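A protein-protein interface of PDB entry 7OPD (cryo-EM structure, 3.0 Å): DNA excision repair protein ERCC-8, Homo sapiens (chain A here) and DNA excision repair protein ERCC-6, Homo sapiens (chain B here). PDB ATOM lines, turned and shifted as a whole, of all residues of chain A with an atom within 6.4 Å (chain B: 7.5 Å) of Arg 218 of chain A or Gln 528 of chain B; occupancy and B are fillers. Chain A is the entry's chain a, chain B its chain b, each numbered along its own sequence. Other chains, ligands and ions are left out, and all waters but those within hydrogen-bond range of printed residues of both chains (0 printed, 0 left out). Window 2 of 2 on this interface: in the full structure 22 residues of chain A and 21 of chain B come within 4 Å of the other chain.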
ATOM      1  N   HIS A 180     -28.553  27.355   8.514  1.00  0.00           N
ATOM      2  CA  HIS A 180     -28.993  26.039   8.107  1.00  0.00           C
ATOM      3  C   HIS A 180     -30.179  25.615   8.927  1.00  0.00           C
ATOM      4  O   HIS A 180     -30.182  25.806  10.126  1.00  0.00           O
ATOM      5  CB  HIS A 180     -27.834  25.107   8.304  1.00  0.00           C
ATOM      6  CG  HIS A 180     -28.114  23.732   7.884  1.00  0.00           C
ATOM      7  ND1 HIS A 180     -28.061  23.323   6.594  1.00  0.00           N
ATOM      8  CD2 HIS A 180     -28.548  22.683   8.584  1.00  0.00           C
ATOM      9  CE1 HIS A 180     -28.423  22.068   6.518  1.00  0.00           C
ATOM     10  NE2 HIS A 180     -28.710  21.650   7.716  1.00  0.00           N
ATOM     11  N   LEU A 182     -33.346  22.549   9.340  1.00  0.00           N
ATOM     12  CA  LEU A 182     -33.933  21.295   8.965  1.00  0.00           C
ATOM     13  C   LEU A 182     -35.405  21.553   9.061  1.00  0.00           C
ATOM     14  O   LEU A 182     -35.867  22.129  10.032  1.00  0.00           O
ATOM     15  CB  LEU A 182     -33.488  20.175   9.882  1.00  0.00           C
ATOM     16  CG  LEU A 182     -32.027  20.134  10.177  1.00  0.00           C
ATOM     17  CD1 LEU A 182     -31.793  19.401  11.336  1.00  0.00           C
ATOM     18  CD2 LEU A 182     -31.403  19.491   9.088  1.00  0.00           C
ATOM     19  N   ILE A 201     -25.726  12.345  12.708  1.00  0.00           N
ATOM     20  CA  ILE A 201     -27.119  12.024  12.927  1.00  0.00           C
ATOM     21  C   ILE A 201     -27.631  12.840  14.101  1.00  0.00           C
ATOM     22  O   ILE A 201     -26.966  12.967  15.115  1.00  0.00           O
ATOM     23  CB  ILE A 201     -27.306  10.539  13.165  1.00  0.00           C
ATOM     24  CG1 ILE A 201     -26.871   9.749  11.968  1.00  0.00           C
ATOM     25  CG2 ILE A 201     -28.682  10.240  13.472  1.00  0.00           C
ATOM     26  CD1 ILE A 201     -27.600   9.907  10.777  1.00  0.00           C
ATOM     27  N   TRP A 214     -32.211  12.854  11.565  1.00  0.00           N
ATOM     28  CA  TRP A 214     -31.713  13.541  10.409  1.00  0.00           C
ATOM     29  C   TRP A 214     -30.259  13.235  10.223  1.00  0.00           C
ATOM     30  O   TRP A 214     -29.525  13.178  11.176  1.00  0.00           O
ATOM     31  CB  TRP A 214     -31.821  15.019  10.571  1.00  0.00           C
ATOM     32  CG  TRP A 214     -33.020  15.509  11.031  1.00  0.00           C
ATOM     33  CD1 TRP A 214     -33.434  15.532  12.267  1.00  0.00           C
ATOM     34  CD2 TRP A 214     -34.007  16.110  10.264  1.00  0.00           C
ATOM     35  NE1 TRP A 214     -34.635  16.080  12.356  1.00  0.00           N
ATOM     36  CE2 TRP A 214     -35.011  16.460  11.108  1.00  0.00           C
ATOM     37  CE3 TRP A 214     -34.135  16.396   8.919  1.00  0.00           C
ATOM     38  CZ2 TRP A 214     -36.107  17.091  10.678  1.00  0.00           C
ATOM     39  CZ3 TRP A 214     -35.191  16.994   8.505  1.00  0.00           C
ATOM     40  CH2 TRP A 214     -36.186  17.349   9.369  1.00  0.00           C
ATOM     41  N   ASP A 215     -29.820  13.187   8.992  1.00  0.00           N
ATOM     42  CA  ASP A 215     -28.416  13.231   8.641  1.00  0.00           C
ATOM     43  C   ASP A 215     -28.158  14.627   8.182  1.00  0.00           C
ATOM     44  O   ASP A 215     -28.425  14.943   7.046  1.00  0.00           O
ATOM     45  CB  ASP A 215     -28.142  12.307   7.597  1.00  0.00           C
ATOM     46  CG  ASP A 215     -26.720  12.290   7.182  1.00  0.00           C
ATOM     47  OD1 ASP A 215     -25.923  13.127   7.553  1.00  0.00           O
ATOM     48  OD2 ASP A 215     -26.380  11.418   6.391  1.00  0.00           O
ATOM     49  N   VAL A 216     -27.618  15.474   9.030  1.00  0.00           N
ATOM     50  CA  VAL A 216     -27.602  16.860   8.687  1.00  0.00           C
ATOM     51  C   VAL A 216     -26.727  17.130   7.500  1.00  0.00           C
ATOM     52  O   VAL A 216     -26.825  18.173   6.905  1.00  0.00           O
ATOM     53  CB  VAL A 216     -27.164  17.681   9.872  1.00  0.00           C
ATOM     54  CG1 VAL A 216     -28.004  17.397  10.982  1.00  0.00           C
ATOM     55  CG2 VAL A 216     -25.819  17.427  10.193  1.00  0.00           C
ATOM     56  N   ARG A 217     -25.809  16.264   7.188  1.00  0.00           N
ATOM     57  CA  ARG A 217     -25.046  16.432   5.978  1.00  0.00           C
ATOM     58  C   ARG A 217     -25.927  16.356   4.777  1.00  0.00           C
ATOM     59  O   ARG A 217     -25.626  16.930   3.747  1.00  0.00           O
ATOM     60  CB  ARG A 217     -24.013  15.339   5.845  1.00  0.00           C
ATOM     61  CG  ARG A 217     -22.792  15.467   6.620  1.00  0.00           C
ATOM     62  CD  ARG A 217     -21.864  14.323   6.380  1.00  0.00           C
ATOM     63  NE  ARG A 217     -22.516  13.056   6.599  1.00  0.00           N
ATOM     64  CZ  ARG A 217     -22.043  11.882   6.230  1.00  0.00           C
ATOM     65  NH1 ARG A 217     -20.889  11.769   5.604  1.00  0.00           N
ATOM     66  NH2 ARG A 217     -22.743  10.803   6.495  1.00  0.00           N
ATOM     67  N   ARG A 218     -26.933  15.541   4.858  1.00  0.00           N
ATOM     68  CA  ARG A 218     -27.783  15.195   3.759  1.00  0.00           C
ATOM     69  C   ARG A 218     -28.665  16.358   3.423  1.00  0.00           C
ATOM     70  O   ARG A 218     -29.087  17.105   4.290  1.00  0.00           O
ATOM     71  CB  ARG A 218     -28.596  14.001   4.185  1.00  0.00           C
ATOM     72  CG  ARG A 218     -29.346  13.350   3.169  1.00  0.00           C
ATOM     73  CD  ARG A 218     -29.846  11.963   3.487  1.00  0.00           C
ATOM     74  NE  ARG A 218     -28.860  11.096   4.108  1.00  0.00           N
ATOM     75  CZ  ARG A 218     -29.029   9.788   4.278  1.00  0.00           C
ATOM     76  NH1 ARG A 218     -30.117   9.177   3.834  1.00  0.00           N
ATOM     77  NH2 ARG A 218     -28.076   9.073   4.839  1.00  0.00           N
ATOM     78  N   ALA A 219     -29.014  16.482   2.174  1.00  0.00           N
ATOM     79  CA  ALA A 219     -29.799  17.618   1.746  1.00  0.00           C
ATOM     80  C   ALA A 219     -31.240  17.247   1.530  1.00  0.00           C
ATOM     81  O   ALA A 219     -31.953  17.972   0.864  1.00  0.00           O
ATOM     82  CB  ALA A 219     -29.247  18.191   0.459  1.00  0.00           C
ATOM     83  N   SER A 220     -31.710  16.183   2.134  1.00  0.00           N
ATOM     84  CA  SER A 220     -32.934  15.592   1.655  1.00  0.00           C
ATOM     85  C   SER A 220     -33.900  15.230   2.745  1.00  0.00           C
ATOM     86  O   SER A 220     -34.747  14.370   2.543  1.00  0.00           O
ATOM     87  CB  SER A 220     -32.622  14.350   0.878  1.00  0.00           C
ATOM     88  OG  SER A 220     -32.077  13.389   1.734  1.00  0.00           O
ATOM     89  N   GLY A 221     -33.867  15.889   3.843  1.00  0.00           N
ATOM     90  CA  GLY A 221     -34.880  15.630   4.830  1.00  0.00           C
ATOM     91  C   GLY A 221     -34.563  14.446   5.713  1.00  0.00           C
ATOM     92  O   GLY A 221     -33.522  13.817   5.626  1.00  0.00           O
ATOM     93  N   CYS A 222     -35.508  14.145   6.573  1.00  0.00           N
ATOM     94  CA  CYS A 222     -35.273  13.220   7.649  1.00  0.00           C
ATOM     95  C   CYS A 222     -34.920  11.873   7.101  1.00  0.00           C
ATOM     96  O   CYS A 222     -35.277  11.554   5.984  1.00  0.00           O
ATOM     97  CB  CYS A 222     -36.501  13.132   8.516  1.00  0.00           C
ATOM     98  SG  CYS A 222     -37.945  12.459   7.807  1.00  0.00           S
ATOM     99  N   LEU A 223     -34.088  11.137   7.828  1.00  0.00           N
ATOM    100  CA  LEU A 223     -33.863   9.734   7.518  1.00  0.00           C
ATOM    101  C   LEU A 223     -35.034   8.883   7.898  1.00  0.00           C
ATOM    102  O   LEU A 223     -35.421   7.987   7.160  1.00  0.00           O
ATOM    103  CB  LEU A 223     -32.674   9.212   8.255  1.00  0.00           C
ATOM    104  CG  LEU A 223     -31.434  10.006   8.109  1.00  0.00           C
ATOM    105  CD1 LEU A 223     -30.400   9.236   8.766  1.00  0.00           C
ATOM    106  CD2 LEU A 223     -31.100  10.197   6.722  1.00  0.00           C
ATOM    107  N   TRP B 522     -17.732  13.691  -6.092  1.00  0.00           N
ATOM    108  CA  TRP B 522     -18.062  12.434  -5.449  1.00  0.00           C
ATOM    109  C   TRP B 522     -18.208  12.594  -3.951  1.00  0.00           C
ATOM    110  O   TRP B 522     -19.058  11.942  -3.352  1.00  0.00           O
ATOM    111  CB  TRP B 522     -17.046  11.351  -5.747  1.00  0.00           C
ATOM    112  CG  TRP B 522     -17.639  10.040  -5.405  1.00  0.00           C
ATOM    113  CD1 TRP B 522     -18.711   9.434  -5.992  1.00  0.00           C
ATOM    114  CD2 TRP B 522     -17.242   9.198  -4.363  1.00  0.00           C
ATOM    115  NE1 TRP B 522     -18.988   8.256  -5.383  1.00  0.00           N
ATOM    116  CE2 TRP B 522     -18.098   8.094  -4.367  1.00  0.00           C
ATOM    117  CE3 TRP B 522     -16.243   9.269  -3.420  1.00  0.00           C
ATOM    118  CZ2 TRP B 522     -17.975   7.090  -3.491  1.00  0.00           C
ATOM    119  CZ3 TRP B 522     -16.126   8.286  -2.559  1.00  0.00           C
ATOM    120  CH2 TRP B 522     -16.981   7.192  -2.592  1.00  0.00           C
ATOM    121  N   GLU B 523     -17.410  13.436  -3.326  1.00  0.00           N
ATOM    122  CA  GLU B 523     -17.605  13.673  -1.909  1.00  0.00           C
ATOM    123  C   GLU B 523     -19.008  14.171  -1.648  1.00  0.00           C
ATOM    124  O   GLU B 523     -19.644  13.773  -0.675  1.00  0.00           O
ATOM    125  CB  GLU B 523     -16.605  14.693  -1.400  1.00  0.00           C
ATOM    126  CG  GLU B 523     -15.169  14.240  -1.434  1.00  0.00           C
ATOM    127  CD  GLU B 523     -14.879  13.113  -0.477  1.00  0.00           C
ATOM    128  OE1 GLU B 523     -15.524  13.052   0.583  1.00  0.00           O
ATOM    129  OE2 GLU B 523     -13.990  12.295  -0.771  1.00  0.00           O
ATOM    130  N   LEU B 524     -19.513  15.050  -2.504  1.00  0.00           N
ATOM    131  CA  LEU B 524     -20.886  15.481  -2.333  1.00  0.00           C
ATOM    132  C   LEU B 524     -21.817  14.315  -2.437  1.00  0.00           C
ATOM    133  O   LEU B 524     -22.683  14.145  -1.594  1.00  0.00           O
ATOM    134  CB  LEU B 524     -21.282  16.512  -3.359  1.00  0.00           C
ATOM    135  CG  LEU B 524     -20.729  17.895  -3.214  1.00  0.00           C
ATOM    136  CD1 LEU B 524     -21.089  18.633  -4.400  1.00  0.00           C
ATOM    137  CD2 LEU B 524     -21.233  18.584  -2.035  1.00  0.00           C
ATOM    138  N   HIS B 525     -21.620  13.469  -3.430  1.00  0.00           N
ATOM    139  CA  HIS B 525     -22.490  12.320  -3.573  1.00  0.00           C
ATOM    140  C   HIS B 525     -22.503  11.501  -2.331  1.00  0.00           C
ATOM    141  O   HIS B 525     -23.512  10.899  -1.987  1.00  0.00           O
ATOM    142  CB  HIS B 525     -22.020  11.473  -4.716  1.00  0.00           C
ATOM    143  CG  HIS B 525     -22.783  10.211  -4.885  1.00  0.00           C
ATOM    144  ND1 HIS B 525     -23.939  10.140  -5.611  1.00  0.00           N
ATOM    145  CD2 HIS B 525     -22.529   8.955  -4.468  1.00  0.00           C
ATOM    146  CE1 HIS B 525     -24.378   8.900  -5.623  1.00  0.00           C
ATOM    147  NE2 HIS B 525     -23.537   8.159  -4.940  1.00  0.00           N
ATOM    148  N   CYS B 526     -21.374  11.421  -1.667  1.00  0.00           N
ATOM    149  CA  CYS B 526     -21.338  10.704  -0.416  1.00  0.00           C
ATOM    150  C   CYS B 526     -22.149  11.414   0.639  1.00  0.00           C
ATOM    151  O   CYS B 526     -22.934  10.787   1.344  1.00  0.00           O
ATOM    152  CB  CYS B 526     -19.904  10.529   0.017  1.00  0.00           C
ATOM    153  SG  CYS B 526     -19.003   9.423  -1.026  1.00  0.00           S
ATOM    154  N   GLN B 527     -22.002  12.717   0.752  1.00  0.00           N
ATOM    155  CA  GLN B 527     -22.836  13.451   1.680  1.00  0.00           C
ATOM    156  C   GLN B 527     -24.288  13.406   1.303  1.00  0.00           C
ATOM    157  O   GLN B 527     -25.124  13.554   2.174  1.00  0.00           O
ATOM    158  CB  GLN B 527     -22.414  14.882   1.714  1.00  0.00           C
ATOM    159  CG  GLN B 527     -21.335  15.127   2.599  1.00  0.00           C
ATOM    160  CD  GLN B 527     -20.511  16.241   2.106  1.00  0.00           C
ATOM    161  OE1 GLN B 527     -19.581  16.029   1.359  1.00  0.00           O
ATOM    162  NE2 GLN B 527     -20.829  17.450   2.519  1.00  0.00           N
ATOM    163  N   GLN B 528     -24.611  13.159   0.045  1.00  0.00           N
ATOM    164  CA  GLN B 528     -25.944  13.348  -0.524  1.00  0.00           C
ATOM    165  C   GLN B 528     -26.348  14.802  -0.486  1.00  0.00           C
ATOM    166  O   GLN B 528     -27.420  15.155  -0.033  1.00  0.00           O
ATOM    167  CB  GLN B 528     -26.980  12.496   0.170  1.00  0.00           C
ATOM    168  CG  GLN B 528     -26.722  11.095   0.024  1.00  0.00           C
ATOM    169  CD  GLN B 528     -27.784  10.292   0.594  1.00  0.00           C
ATOM    170  OE1 GLN B 528     -27.695   9.891   1.728  1.00  0.00           O
ATOM    171  NE2 GLN B 528     -28.793  10.002  -0.182  1.00  0.00           N
ATOM    172  N   ALA B 529     -25.481  15.650  -0.987  1.00  0.00           N
ATOM    173  CA  ALA B 529     -25.721  17.068  -1.088  1.00  0.00           C
ATOM    174  C   ALA B 529     -25.407  17.486  -2.498  1.00  0.00           C
ATOM    175  O   ALA B 529     -24.881  16.713  -3.277  1.00  0.00           O
ATOM    176  CB  ALA B 529     -24.883  17.844  -0.112  1.00  0.00           C
ATOM    177  N   GLY B 530     -25.823  18.672  -2.845  1.00  0.00           N
ATOM    178  CA  GLY B 530     -25.630  19.195  -4.171  1.00  0.00           C
ATOM    179  C   GLY B 530     -24.605  20.255  -4.128  1.00  0.00           C
ATOM    180  O   GLY B 530     -24.200  20.687  -3.075  1.00  0.00           O
ATOM    181  N   ARG B 565     -31.210   0.424  -4.135  1.00  0.00           N
ATOM    182  CA  ARG B 565     -32.121   1.111  -5.032  1.00  0.00           C
ATOM    183  C   ARG B 565     -31.525   1.160  -6.420  1.00  0.00           C
ATOM    184  O   ARG B 565     -32.104   0.630  -7.363  1.00  0.00           O
ATOM    185  CB  ARG B 565     -32.414   2.526  -4.534  1.00  0.00           C
ATOM    186  CG  ARG B 565     -33.134   2.560  -3.188  1.00  0.00           C
ATOM    187  CD  ARG B 565     -32.626   3.646  -2.263  1.00  0.00           C
ATOM    188  NE  ARG B 565     -31.176   3.614  -2.109  1.00  0.00           N
ATOM    189  CZ  ARG B 565     -30.512   2.753  -1.347  1.00  0.00           C
ATOM    190  NH1 ARG B 565     -31.150   1.823  -0.652  1.00  0.00           N
ATOM    191  NH2 ARG B 565     -29.191   2.819  -1.285  1.00  0.00           N
ATOM    192  N   TYR B 645     -29.825  11.981 -10.737  1.00  0.00           N
ATOM    193  CA  TYR B 645     -29.107  13.233 -10.785  1.00  0.00           C
ATOM    194  C   TYR B 645     -29.855  14.230 -11.621  1.00  0.00           C
ATOM    195  O   TYR B 645     -30.477  13.877 -12.613  1.00  0.00           O
ATOM    196  CB  TYR B 645     -27.739  13.137 -11.364  1.00  0.00           C
ATOM    197  CG  TYR B 645     -26.760  12.773 -10.363  1.00  0.00           C
ATOM    198  CD1 TYR B 645     -26.823  11.603  -9.733  1.00  0.00           C
ATOM    199  CD2 TYR B 645     -25.762  13.616 -10.049  1.00  0.00           C
ATOM    200  CE1 TYR B 645     -25.951  11.290  -8.821  1.00  0.00           C
ATOM    201  CE2 TYR B 645     -24.891  13.313  -9.137  1.00  0.00           C
ATOM    202  CZ  TYR B 645     -24.996  12.140  -8.515  1.00  0.00           C
ATOM    203  OH  TYR B 645     -24.118  11.747  -7.589  1.00  0.00           O
ATOM    204  N   THR B 670     -34.419  14.157  -5.703  1.00  0.00           N
ATOM    205  CA  THR B 670     -33.177  13.558  -5.312  1.00  0.00           C
ATOM    206  C   THR B 670     -32.259  14.580  -4.705  1.00  0.00           C
ATOM    207  O   THR B 670     -32.342  15.734  -5.049  1.00  0.00           O
ATOM    208  CB  THR B 670     -32.521  12.988  -6.506  1.00  0.00           C
ATOM    209  OG1 THR B 670     -33.545  12.357  -7.264  1.00  0.00           O
ATOM    210  CG2 THR B 670     -31.528  11.994  -6.106  1.00  0.00           C
ATOM    211  N   PRO B 671     -31.370  14.178  -3.810  1.00  0.00           N
ATOM    212  CA  PRO B 671     -30.409  15.106  -3.258  1.00  0.00           C
ATOM    213  C   PRO B 671     -29.289  15.438  -4.160  1.00  0.00           C
ATOM    214  O   PRO B 671     -28.519  16.333  -3.856  1.00  0.00           O
ATOM    215  CB  PRO B 671     -29.892  14.370  -2.052  1.00  0.00           C
ATOM    216  CG  PRO B 671     -30.224  13.127  -2.243  1.00  0.00           C
ATOM    217  CD  PRO B 671     -31.426  13.018  -2.959  1.00  0.00           C
ATOM    218  N   HIS B 672     -29.123  14.723  -5.236  1.00  0.00           N
ATOM    219  CA  HIS B 672     -27.985  14.910  -6.092  1.00  0.00           C
ATOM    220  C   HIS B 672     -28.416  15.869  -7.147  1.00  0.00           C
ATOM    221  O   HIS B 672     -28.759  15.519  -8.259  1.00  0.00           O
ATOM    222  CB  HIS B 672     -27.528  13.598  -6.662  1.00  0.00           C
ATOM    223  CG  HIS B 672     -27.312  12.558  -5.633  1.00  0.00           C
ATOM    224  ND1 HIS B 672     -26.210  12.520  -4.833  1.00  0.00           N
ATOM    225  CD2 HIS B 672     -28.103  11.553  -5.238  1.00  0.00           C
ATOM    226  CE1 HIS B 672     -26.317  11.504  -4.007  1.00  0.00           C
ATOM    227  NE2 HIS B 672     -27.458  10.901  -4.235  1.00  0.00           N
ATOM    228  N   ARG B 673     -28.426  17.107  -6.746  1.00  0.00           N
ATOM    229  CA  ARG B 673     -28.690  18.235  -7.598  1.00  0.00           C
ATOM    230  C   ARG B 673     -27.383  18.939  -7.827  1.00  0.00           C
ATOM    231  O   ARG B 673     -26.658  19.177  -6.873  1.00  0.00           O
ATOM    232  CB  ARG B 673     -29.627  19.193  -6.914  1.00  0.00           C
ATOM    233  CG  ARG B 673     -31.025  19.101  -7.233  1.00  0.00           C
ATOM    234  CD  ARG B 673     -31.764  18.185  -6.554  1.00  0.00           C
ATOM    235  NE  ARG B 673     -31.791  18.415  -5.143  1.00  0.00           N
ATOM    236  CZ  ARG B 673     -32.690  19.120  -4.496  1.00  0.00           C
ATOM    237  NH1 ARG B 673     -33.700  19.722  -5.109  1.00  0.00           N
ATOM    238  NH2 ARG B 673     -32.588  19.165  -3.185  1.00  0.00           N
ATOM    239  N   ILE B 695     -29.808  23.496  -4.846  1.00  0.00           N
ATOM    240  CA  ILE B 695     -28.876  22.428  -4.574  1.00  0.00           C
ATOM    241  C   ILE B 695     -29.051  21.893  -3.180  1.00  0.00           C
ATOM    242  O   ILE B 695     -29.024  20.690  -2.979  1.00  0.00           O
ATOM    243  CB  ILE B 695     -27.430  22.832  -4.819  1.00  0.00           C
ATOM    244  CG1 ILE B 695     -27.005  23.972  -3.978  1.00  0.00           C
ATOM    245  CG2 ILE B 695     -27.304  23.166  -6.183  1.00  0.00           C
ATOM    246  CD1 ILE B 695     -25.656  24.022  -3.838  1.00  0.00           C
ATOM    247  N   PHE B 696     -29.247  22.751  -2.203  1.00  0.00           N
ATOM    248  CA  PHE B 696     -29.213  22.342  -0.816  1.00  0.00           C
ATOM    249  C   PHE B 696     -30.324  23.082  -0.107  1.00  0.00           C
ATOM    250  O   PHE B 696     -30.080  24.110   0.510  1.00  0.00           O
ATOM    251  CB  PHE B 696     -27.875  22.680  -0.198  1.00  0.00           C
ATOM    252  CG  PHE B 696     -27.643  21.995   1.049  1.00  0.00           C
ATOM    253  CD1 PHE B 696     -28.327  22.356   2.104  1.00  0.00           C
ATOM    254  CD2 PHE B 696     -26.933  20.861   1.140  1.00  0.00           C
ATOM    255  CE1 PHE B 696     -28.208  21.760   3.209  1.00  0.00           C
ATOM    256  CE2 PHE B 696     -26.811  20.272   2.318  1.00  0.00           C
ATOM    257  CZ  PHE B 696     -27.470  20.714   3.329  1.00  0.00           C
ATOM    258  N   PRO B 697     -31.528  22.539  -0.078  1.00  0.00           N
ATOM    259  CA  PRO B 697     -32.668  23.351   0.287  1.00  0.00           C
ATOM    260  C   PRO B 697     -32.662  23.999   1.633  1.00  0.00           C
ATOM    261  O   PRO B 697     -33.402  24.952   1.811  1.00  0.00           O
ATOM    262  CB  PRO B 697     -33.798  22.368   0.161  1.00  0.00           C
ATOM    263  CG  PRO B 697     -33.406  21.576  -0.833  1.00  0.00           C
ATOM    264  CD  PRO B 697     -32.010  21.351  -0.752  1.00  0.00           C
ATOM    265  N   GLY B 698     -31.882  23.598   2.575  1.00  0.00           N
ATOM    266  CA  GLY B 698     -31.944  24.314   3.826  1.00  0.00           C
ATOM    267  C   GLY B 698     -30.781  25.183   4.183  1.00  0.00           C
ATOM    268  O   GLY B 698     -30.909  25.925   5.110  1.00  0.00           O
ATOM    269  N   LYS B 699     -29.663  25.118   3.490  1.00  0.00           N
ATOM    270  CA  LYS B 699     -28.422  25.616   4.034  1.00  0.00           C
ATOM    271  C   LYS B 699     -28.512  27.076   4.387  1.00  0.00           C
ATOM    272  O   LYS B 699     -28.216  27.479   5.506  1.00  0.00           O
ATOM    273  CB  LYS B 699     -27.303  25.408   3.052  1.00  0.00           C
ATOM    274  CG  LYS B 699     -25.973  25.723   3.523  1.00  0.00           C
ATOM    275  CD  LYS B 699     -25.508  24.993   4.735  1.00  0.00           C
ATOM    276  CE  LYS B 699     -25.474  23.553   4.560  1.00  0.00           C
ATOM    277  NZ  LYS B 699     -24.503  22.982   5.486  1.00  0.00           N
ATOM    278  N   TYR B 744     -19.947  23.677  -0.880  1.00  0.00           N
ATOM    279  CA  TYR B 744     -20.890  23.355  -1.915  1.00  0.00           C
ATOM    280  C   TYR B 744     -20.722  24.178  -3.145  1.00  0.00           C
ATOM    281  O   TYR B 744     -21.512  24.052  -4.060  1.00  0.00           O
ATOM    282  CB  TYR B 744     -22.280  23.517  -1.384  1.00  0.00           C
ATOM    283  CG  TYR B 744     -22.447  22.881  -0.099  1.00  0.00           C
ATOM    284  CD1 TYR B 744     -22.647  21.567  -0.020  1.00  0.00           C
ATOM    285  CD2 TYR B 744     -22.358  23.580   1.029  1.00  0.00           C
ATOM    286  CE1 TYR B 744     -22.772  20.995   1.099  1.00  0.00           C
ATOM    287  CE2 TYR B 744     -22.458  23.004   2.153  1.00  0.00           C
ATOM    288  CZ  TYR B 744     -22.678  21.700   2.188  1.00  0.00           C
ATOM    289  OH  TYR B 744     -22.811  21.050   3.359  1.00  0.00           O
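The backbone carbonyl oxygen (O) of Gln 528 of chain B lies within hydrogen-bond range of the backbone NH (N) of Ala 219 of chain A, 3.0 Å away.
The guanidinium group (NE) of Arg 218 of chain A lies close to the side-chain amide oxygen (OE1) of Gln 528 of chain B, at 2.9 Å.
The backbone NH of His 180 of chain A sits at hydrogen-bond distance from the backbone carbonyl oxygen of Lys 699 of chain B.
The side-chain amino group (NZ) of Lys 699 of chain B lies within hydrogen-bond range of the side-chain hydroxyl (OH) of Tyr 744 of chain B (3.3 Å).
The side-chain carboxylate (OD1) of Asp 215 of chain A is in salt-bridge range of the guanidinium group (NE) of Arg 217 of chain A (3.5 Å).
The backbone carbonyl oxygen (O) of Glu 523 of chain B lies close to the side-chain amide oxygen (OE1) of Gln 527 of chain B, at 3.0 Å.
The side-chain carboxylate (OD2) of Asp 215 of chain A lies within salt-bridge range of the guanidinium group (NH2) of Arg 218 of chain A (3.3 Å).
Among the printed residues, merely in contact across the chains: His 180 of chain A with Phe 696 of chain B, Arg 218 of chain A with Gln 527 of chain B, His 180 of chain A with Gly 698 of chain B, Ala 219 of chain A with Phe 696 of chain B, Ala 219 of chain A with Pro 697 of chain B, Arg 217 of chain A with Gln 527 of chain B and Arg 217 of chain A with Phe 696 of chain B.
Printed residues of chain B within 4 Å of His 180 of chain A: Phe 696 (3.3 Å), Gly 698 (3.6 Å) and Lys 699 (3.0 Å).
Of the printed residues of chain B, Arg 217 of chain A touches Gln 527 (3.8 Å) and Phe 696 (3.8 Å).
Printed residues of chain B within 4 Å of Arg 218 of chain A: Gln 527 (3.5 Å) and Gln 528 (2.9 Å).
Of the printed residues of chain A, Gln 527 of chain B touches Arg 217 (3.8 Å) and Arg 218 (3.5 Å).
Of chain A, only Arg 218 and Ala 219 come within 4 Å of Gln 528 of chain B.
Arg 673 of chain B touches none of the printed residues of chain A.
Printed residues of chain A within 4 Å of Phe 696 of chain B: His 180 (3.3 Å), Arg 217 (3.8 Å) and Ala 219 (3.6 Å).
Printed residues of chain A within 4 Å of Gly 698 of chain B: His 180 (3.6 Å).
The nearest residue of chain B that does not touch Arg 218 of chain A is Phe 696 of chain B (4.1 Å).
The nearest printed residue of chain A that does not touch Lys 699 of chain B is Val 216 of chain A (5.5 Å).
Of the 21 printed residues of chain B, 6 touch a printed residue of chain A.
Printed residues of chain B that touch a printed residue of chain A: Gln 527, Gln 528, Phe 696, Pro 697, Gly 698 and Lys 699.
Printed residues of chain A that touch a printed residue of chain B: His 180, Arg 217, Arg 218 and Ala 219.
Hydrophobic or aromatic side chains of chain A that line the printed part of chain B: His 180 and Ala 219.
Along chain A the printed residues that touch a printed residue of chain B span positions 180 to 219.
Among the printed residues, no Asp or Glu carboxylate lies within 4 Å of a Lys or Arg side-chain nitrogen of the other chain.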
